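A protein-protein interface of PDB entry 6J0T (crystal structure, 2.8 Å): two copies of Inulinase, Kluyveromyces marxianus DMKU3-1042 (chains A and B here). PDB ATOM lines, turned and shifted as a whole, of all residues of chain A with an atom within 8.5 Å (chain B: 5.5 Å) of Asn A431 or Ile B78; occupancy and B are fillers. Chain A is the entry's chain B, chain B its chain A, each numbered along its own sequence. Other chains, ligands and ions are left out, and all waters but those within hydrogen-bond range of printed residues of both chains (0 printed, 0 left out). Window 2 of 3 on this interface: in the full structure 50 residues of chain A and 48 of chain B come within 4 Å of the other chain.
NE2 of Gln B340 lies within hydrogen-bond range of O of Val A432. The side-chain amide nitrogen (NE2) of Gln B339 sits at hydrogen-bond distance from the side-chain hydroxyl (OG) of Ser A430.
The side-chain carboxylate (OE2) of Glu A455 is in hydrogen-bond range of the backbone NH (N) of Asn A457. NE of Arg B347 is in hydrogen-bond range of O of Gln B339, 3.2 Å away. The side-chain amide oxygen (OE1) of Gln B339 is in hydrogen-bond range of the backbone NH (N) of Trp B79, at 2.6 Å. The backbone carbonyl oxygen (O) of Ile B78 lies within hydrogen-bond range of the side-chain amide nitrogen (ND2) of Asn B73. The backbone carbonyl oxygen of Thr B77 lies within hydrogen-bond range of the guanidinium group of Arg B347, at 2.8 Å.
Among the printed residues, pairs that only touch across the chains: Ser A430 with Gln B340 (3.5 Å), Asn A431 with Ile B78 (3.6 Å), Asn A431 with Gln B339 (3.1 Å), Asn A431 with Gln B340 (3.7 Å), Asn A431 with Arg B347 (3.7 Å), Phe A433 with Gln B340 (3.8 Å) and Asn A457 with Gln B340 (3.8 Å).
Printed residues of chain B within 4 Å of Asn A431: Ile B78, Gln B339, Gln B340 and Arg B347. Of chain A, only Asn A431 (3.6 Å) comes within 4 Å of Ile B78. Of the printed residues of chain A, Arg B347 touches Asn A431 (3.7 Å). Of the printed residues of chain B, Asn A457 touches Gln B340. Ala B76 touches none of the printed residues of chain A. The nearest residue of chain B that does not touch Asn A431 is Thr B77 (5.3 Å). The nearest residue of chain A that does not touch Ile B78 is Ser A430 (4.1 Å). The nearest printed residue of chain B that does not touch Ser A430 is Ile B78 (4.1 Å).
Printed residues of chain A that touch a printed residue of chain B: Ser A430, Asn A431, Val A432, Phe A433 and Asn A457. Of the 10 printed residues of chain B, 4 touch a printed residue of chain A. Hydrophobic or aromatic side chains of chain B within 4 Å of the printed part of chain A: Ile B78. Along chain B the printed residues that touch a printed residue of chain A span positions 78 to 347. Among the printed residues, 9 pairs touch across the chains. Among the printed residues, no Asp or Glu carboxylate lies within 4 Å of a Lys or Arg side-chain nitrogen of the other chain.
No position is printed for both chains. Of the 9 pairs that touch across the chains among the printed residues, none has its exchanged pair printed and touching as well.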
ATOM      1  N   ASP A 427     -14.078 -16.390  -0.398  1.00  0.00           N
ATOM      2  CA  ASP A 427     -13.674 -17.345   0.621  1.00  0.00           C
ATOM      3  C   ASP A 427     -14.848 -17.998   1.362  1.00  0.00           C
ATOM      4  O   ASP A 427     -14.609 -18.786   2.281  1.00  0.00           O
ATOM      5  CB  ASP A 427     -12.728 -16.667   1.627  1.00  0.00           C
ATOM      6  CG  ASP A 427     -11.513 -16.018   0.961  1.00  0.00           C
ATOM      7  OD1 ASP A 427     -10.619 -16.751   0.470  1.00  0.00           O
ATOM      8  OD2 ASP A 427     -11.453 -14.768   0.936  1.00  0.00           O
ATOM      9  N   ILE A 428     -16.095 -17.721   0.985  1.00  0.00           N
ATOM     10  CA  ILE A 428     -17.264 -18.282   1.662  1.00  0.00           C
ATOM     11  C   ILE A 428     -17.918 -19.316   0.756  1.00  0.00           C
ATOM     12  O   ILE A 428     -18.444 -18.966  -0.309  1.00  0.00           O
ATOM     13  CB  ILE A 428     -18.279 -17.194   2.036  1.00  0.00           C
ATOM     14  CG1 ILE A 428     -17.794 -16.397   3.243  1.00  0.00           C
ATOM     15  CG2 ILE A 428     -19.630 -17.800   2.329  1.00  0.00           C
ATOM     16  CD1 ILE A 428     -18.568 -15.137   3.459  1.00  0.00           C
ATOM     17  N   LYS A 429     -17.906 -20.586   1.179  1.00  0.00           N
ATOM     18  CA  LYS A 429     -18.752 -21.588   0.530  1.00  0.00           C
ATOM     19  C   LYS A 429     -19.598 -22.350   1.557  1.00  0.00           C
ATOM     20  O   LYS A 429     -19.655 -21.962   2.726  1.00  0.00           O
ATOM     21  CB  LYS A 429     -17.917 -22.534  -0.354  1.00  0.00           C
ATOM     22  CG  LYS A 429     -16.475 -22.765   0.066  1.00  0.00           C
ATOM     23  CD  LYS A 429     -15.780 -23.740  -0.900  1.00  0.00           C
ATOM     24  CE  LYS A 429     -14.281 -23.908  -0.597  1.00  0.00           C
ATOM     25  NZ  LYS A 429     -13.877 -25.354  -0.442  1.00  0.00           N
ATOM     26  N   SER A 430     -20.289 -23.409   1.125  1.00  0.00           N
ATOM     27  CA  SER A 430     -21.342 -24.013   1.933  1.00  0.00           C
ATOM     28  C   SER A 430     -20.837 -24.699   3.196  1.00  0.00           C
ATOM     29  O   SER A 430     -21.660 -25.083   4.031  1.00  0.00           O
ATOM     30  CB  SER A 430     -22.129 -25.029   1.099  1.00  0.00           C
ATOM     31  OG  SER A 430     -23.098 -24.399   0.288  1.00  0.00           O
ATOM     32  N   ASN A 431     -19.538 -24.886   3.366  1.00  0.00           N
ATOM     33  CA  ASN A 431     -19.029 -25.704   4.464  1.00  0.00           C
ATOM     34  C   ASN A 431     -18.262 -24.881   5.489  1.00  0.00           C
ATOM     35  O   ASN A 431     -17.242 -25.327   6.015  1.00  0.00           O
ATOM     36  CB  ASN A 431     -18.151 -26.845   3.947  1.00  0.00           C
ATOM     37  CG  ASN A 431     -16.965 -26.354   3.123  1.00  0.00           C
ATOM     38  OD1 ASN A 431     -16.870 -25.171   2.774  1.00  0.00           O
ATOM     39  ND2 ASN A 431     -16.059 -27.269   2.799  1.00  0.00           N
ATOM     40  N   VAL A 432     -18.755 -23.678   5.801  1.00  0.00           N
ATOM     41  CA  VAL A 432     -18.100 -22.801   6.762  1.00  0.00           C
ATOM     42  C   VAL A 432     -19.147 -21.997   7.519  1.00  0.00           C
ATOM     43  O   VAL A 432     -20.270 -21.796   7.052  1.00  0.00           O
ATOM     44  CB  VAL A 432     -17.097 -21.828   6.097  1.00  0.00           C
ATOM     45  CG1 VAL A 432     -15.775 -22.535   5.787  1.00  0.00           C
ATOM     46  CG2 VAL A 432     -17.712 -21.156   4.872  1.00  0.00           C
ATOM     47  N   PHE A 433     -18.757 -21.518   8.696  1.00  0.00           N
ATOM     48  CA  PHE A 433     -19.603 -20.635   9.485  1.00  0.00           C
ATOM     49  C   PHE A 433     -19.177 -19.199   9.183  1.00  0.00           C
ATOM     50  O   PHE A 433     -18.185 -18.700   9.726  1.00  0.00           O
ATOM     51  CB  PHE A 433     -19.536 -20.965  10.976  1.00  0.00           C
ATOM     52  CG  PHE A 433     -20.778 -20.551  11.721  1.00  0.00           C
ATOM     53  CD1 PHE A 433     -21.998 -21.178  11.460  1.00  0.00           C
ATOM     54  CD2 PHE A 433     -20.748 -19.495  12.618  1.00  0.00           C
ATOM     55  CE1 PHE A 433     -23.143 -20.779  12.109  1.00  0.00           C
ATOM     56  CE2 PHE A 433     -21.897 -19.096  13.276  1.00  0.00           C
ATOM     57  CZ  PHE A 433     -23.094 -19.731  13.015  1.00  0.00           C
ATOM     58  N   ALA A 434     -19.948 -18.540   8.322  1.00  0.00           N
ATOM     59  CA  ALA A 434     -19.683 -17.193   7.829  1.00  0.00           C
ATOM     60  C   ALA A 434     -20.652 -16.239   8.520  1.00  0.00           C
ATOM     61  O   ALA A 434     -21.627 -15.757   7.927  1.00  0.00           O
ATOM     62  CB  ALA A 434     -19.838 -17.158   6.296  1.00  0.00           C
ATOM     63  N   GLU A 455     -26.137 -15.676  10.049  1.00  0.00           N
ATOM     64  CA  GLU A 455     -25.210 -16.490   9.285  1.00  0.00           C
ATOM     65  C   GLU A 455     -25.860 -16.907   7.980  1.00  0.00           C
ATOM     66  O   GLU A 455     -27.066 -17.224   7.939  1.00  0.00           O
ATOM     67  CB  GLU A 455     -24.753 -17.711  10.058  1.00  0.00           C
ATOM     68  CG  GLU A 455     -23.439 -18.247   9.538  1.00  0.00           C
ATOM     69  CD  GLU A 455     -23.683 -19.194   8.397  1.00  0.00           C
ATOM     70  OE1 GLU A 455     -24.387 -20.224   8.579  1.00  0.00           O
ATOM     71  OE2 GLU A 455     -23.179 -18.902   7.291  1.00  0.00           O
ATOM     72  N   ASN A 457     -25.060 -19.373   5.583  1.00  0.00           N
ATOM     73  CA  ASN A 457     -25.318 -20.761   5.209  1.00  0.00           C
ATOM     74  C   ASN A 457     -26.534 -21.322   5.922  1.00  0.00           C
ATOM     75  O   ASN A 457     -27.204 -22.219   5.392  1.00  0.00           O
ATOM     76  CB  ASN A 457     -24.100 -21.635   5.503  1.00  0.00           C
ATOM     77  CG  ASN A 457     -22.883 -21.180   4.763  1.00  0.00           C
ATOM     78  OD1 ASN A 457     -22.935 -20.897   3.564  1.00  0.00           O
ATOM     79  ND2 ASN A 457     -21.774 -21.088   5.471  1.00  0.00           N
ATOM     80  N   TYR A 540     -14.858 -13.495   8.017  1.00  0.00           N
ATOM     81  CA  TYR A 540     -14.608 -13.185   6.596  1.00  0.00           C
ATOM     82  C   TYR A 540     -14.708 -11.673   6.469  1.00  0.00           C
ATOM     83  O   TYR A 540     -15.785 -11.155   6.669  1.00  0.00           O
ATOM     84  CB  TYR A 540     -15.608 -13.956   5.736  1.00  0.00           C
ATOM     85  CG  TYR A 540     -15.420 -15.450   5.789  1.00  0.00           C
ATOM     86  CD1 TYR A 540     -15.882 -16.201   6.853  1.00  0.00           C
ATOM     87  CD2 TYR A 540     -14.728 -16.109   4.800  1.00  0.00           C
ATOM     88  CE1 TYR A 540     -15.671 -17.565   6.923  1.00  0.00           C
ATOM     89  CE2 TYR A 540     -14.502 -17.467   4.853  1.00  0.00           C
ATOM     90  CZ  TYR A 540     -14.969 -18.193   5.920  1.00  0.00           C
ATOM     91  OH  TYR A 540     -14.738 -19.528   5.945  1.00  0.00           O
ATOM     92  N   TRP B  50     -21.339 -35.826  -1.520  1.00  0.00           N
ATOM     93  CA  TRP B  50     -22.410 -35.182  -0.737  1.00  0.00           C
ATOM     94  C   TRP B  50     -23.713 -35.902  -1.027  1.00  0.00           C
ATOM     95  O   TRP B  50     -24.028 -36.027  -2.166  1.00  0.00           O
ATOM     96  CB  TRP B  50     -22.510 -33.741  -1.188  1.00  0.00           C
ATOM     97  CG  TRP B  50     -23.839 -33.154  -0.871  1.00  0.00           C
ATOM     98  CD1 TRP B  50     -24.902 -33.000  -1.700  1.00  0.00           C
ATOM     99  CD2 TRP B  50     -24.245 -32.657   0.398  1.00  0.00           C
ATOM    100  NE1 TRP B  50     -25.930 -32.419  -1.036  1.00  0.00           N
ATOM    101  CE2 TRP B  50     -25.560 -32.212   0.256  1.00  0.00           C
ATOM    102  CE3 TRP B  50     -23.614 -32.543   1.627  1.00  0.00           C
ATOM    103  CZ2 TRP B  50     -26.256 -31.664   1.316  1.00  0.00           C
ATOM    104  CZ3 TRP B  50     -24.306 -32.009   2.674  1.00  0.00           C
ATOM    105  CH2 TRP B  50     -25.610 -31.579   2.519  1.00  0.00           C
ATOM    106  N   ASN B  73     -23.811 -35.356  -4.999  1.00  0.00           N
ATOM    107  CA  ASN B  73     -22.734 -34.642  -5.671  1.00  0.00           C
ATOM    108  C   ASN B  73     -21.476 -35.488  -5.512  1.00  0.00           C
ATOM    109  O   ASN B  73     -20.824 -35.440  -4.455  1.00  0.00           O
ATOM    110  CB  ASN B  73     -22.538 -33.245  -5.074  1.00  0.00           C
ATOM    111  CG  ASN B  73     -21.270 -32.552  -5.592  1.00  0.00           C
ATOM    112  OD1 ASN B  73     -20.599 -33.060  -6.498  1.00  0.00           O
ATOM    113  ND2 ASN B  73     -20.954 -31.379  -5.032  1.00  0.00           N
ATOM    114  N   ALA B  76     -17.698 -33.724  -4.560  1.00  0.00           N
ATOM    115  CA  ALA B  76     -17.295 -33.058  -3.322  1.00  0.00           C
ATOM    116  C   ALA B  76     -18.274 -33.409  -2.206  1.00  0.00           C
ATOM    117  O   ALA B  76     -19.242 -34.139  -2.407  1.00  0.00           O
ATOM    118  CB  ALA B  76     -17.215 -31.535  -3.505  1.00  0.00           C
ATOM    119  N   THR B  77     -18.013 -32.860  -1.021  1.00  0.00           N
ATOM    120  CA  THR B  77     -18.866 -33.071   0.138  1.00  0.00           C
ATOM    121  C   THR B  77     -19.585 -31.776   0.506  1.00  0.00           C
ATOM    122  O   THR B  77     -19.608 -31.367   1.675  1.00  0.00           O
ATOM    123  CB  THR B  77     -18.047 -33.593   1.324  1.00  0.00           C
ATOM    124  OG1 THR B  77     -16.959 -32.709   1.573  1.00  0.00           O
ATOM    125  CG2 THR B  77     -17.502 -34.998   1.028  1.00  0.00           C
ATOM    126  N   ILE B  78     -20.132 -31.115  -0.517  1.00  0.00           N
ATOM    127  CA  ILE B  78     -21.089 -30.025  -0.388  1.00  0.00           C
ATOM    128  C   ILE B  78     -21.931 -30.055  -1.651  1.00  0.00           C
ATOM    129  O   ILE B  78     -21.472 -30.518  -2.702  1.00  0.00           O
ATOM    130  CB  ILE B  78     -20.425 -28.635  -0.242  1.00  0.00           C
ATOM    131  CG1 ILE B  78     -19.438 -28.416  -1.393  1.00  0.00           C
ATOM    132  CG2 ILE B  78     -19.822 -28.416   1.146  1.00  0.00           C
ATOM    133  CD1 ILE B  78     -18.928 -27.048  -1.481  1.00  0.00           C
ATOM    134  N   TRP B  79     -23.152 -29.527  -1.558  1.00  0.00           N
ATOM    135  CA  TRP B  79     -24.082 -29.533  -2.687  1.00  0.00           C
ATOM    136  C   TRP B  79     -23.482 -28.828  -3.916  1.00  0.00           C
ATOM    137  O   TRP B  79     -22.853 -27.767  -3.798  1.00  0.00           O
ATOM    138  CB  TRP B  79     -25.386 -28.861  -2.235  1.00  0.00           C
ATOM    139  CG  TRP B  79     -26.552 -29.020  -3.137  1.00  0.00           C
ATOM    140  CD1 TRP B  79     -27.571 -29.922  -3.015  1.00  0.00           C
ATOM    141  CD2 TRP B  79     -26.844 -28.234  -4.294  1.00  0.00           C
ATOM    142  NE1 TRP B  79     -28.473 -29.757  -4.035  1.00  0.00           N
ATOM    143  CE2 TRP B  79     -28.050 -28.725  -4.837  1.00  0.00           C
ATOM    144  CE3 TRP B  79     -26.190 -27.173  -4.943  1.00  0.00           C
ATOM    145  CZ2 TRP B  79     -28.624 -28.183  -6.001  1.00  0.00           C
ATOM    146  CZ3 TRP B  79     -26.762 -26.637  -6.093  1.00  0.00           C
ATOM    147  CH2 TRP B  79     -27.965 -27.144  -6.612  1.00  0.00           C
ATOM    148  N   GLY B  80     -23.659 -29.428  -5.101  1.00  0.00           N
ATOM    149  CA  GLY B  80     -23.145 -28.821  -6.322  1.00  0.00           C
ATOM    150  C   GLY B  80     -23.635 -29.498  -7.591  1.00  0.00           C
ATOM    151  O   GLY B  80     -24.148 -30.624  -7.576  1.00  0.00           O
ATOM    152  N   GLN B 339     -24.001 -29.107   5.377  1.00  0.00           N
ATOM    153  CA  GLN B 339     -22.783 -29.089   4.546  1.00  0.00           C
ATOM    154  C   GLN B 339     -21.541 -28.766   5.366  1.00  0.00           C
ATOM    155  O   GLN B 339     -20.501 -28.742   4.771  1.00  0.00           O
ATOM    156  CB  GLN B 339     -22.960 -28.086   3.425  1.00  0.00           C
ATOM    157  CG  GLN B 339     -24.281 -28.258   2.714  1.00  0.00           C
ATOM    158  CD  GLN B 339     -24.395 -27.518   1.416  1.00  0.00           C
ATOM    159  OE1 GLN B 339     -23.929 -27.965   0.390  1.00  0.00           O
ATOM    160  NE2 GLN B 339     -25.076 -26.398   1.449  1.00  0.00           N
ATOM    161  N   GLN B 340     -21.661 -28.409   6.640  1.00  0.00           N
ATOM    162  CA  GLN B 340     -20.476 -28.138   7.473  1.00  0.00           C
ATOM    163  C   GLN B 340     -20.252 -29.269   8.464  1.00  0.00           C
ATOM    164  O   GLN B 340     -19.346 -29.148   9.258  1.00  0.00           O
ATOM    165  CB  GLN B 340     -20.668 -26.873   8.273  1.00  0.00           C
ATOM    166  CG  GLN B 340     -21.291 -25.779   7.470  1.00  0.00           C
ATOM    167  CD  GLN B 340     -21.616 -24.677   8.418  1.00  0.00           C
ATOM    168  OE1 GLN B 340     -20.964 -24.527   9.431  1.00  0.00           O
ATOM    169  NE2 GLN B 340     -22.647 -23.922   8.098  1.00  0.00           N
ATOM    170  N   ARG B 347     -20.752 -36.844   3.352  1.00  0.00           N
ATOM    171  CA  ARG B 347     -21.368 -35.927   4.338  1.00  0.00           C
ATOM    172  C   ARG B 347     -22.730 -36.340   4.890  1.00  0.00           C
ATOM    173  O   ARG B 347     -22.781 -36.705   6.064  1.00  0.00           O
ATOM    174  CB  ARG B 347     -21.242 -34.457   3.993  1.00  0.00           C
ATOM    175  CG  ARG B 347     -20.177 -33.820   4.855  1.00  0.00           C
ATOM    176  CD  ARG B 347     -20.397 -32.381   5.162  1.00  0.00           C
ATOM    177  NE  ARG B 347     -19.364 -31.672   4.471  1.00  0.00           N
ATOM    178  CZ  ARG B 347     -18.368 -31.087   5.072  1.00  0.00           C
ATOM    179  NH1 ARG B 347     -17.448 -30.480   4.362  1.00  0.00           N
ATOM    180  NH2 ARG B 347     -18.284 -31.111   6.378  1.00  0.00           N
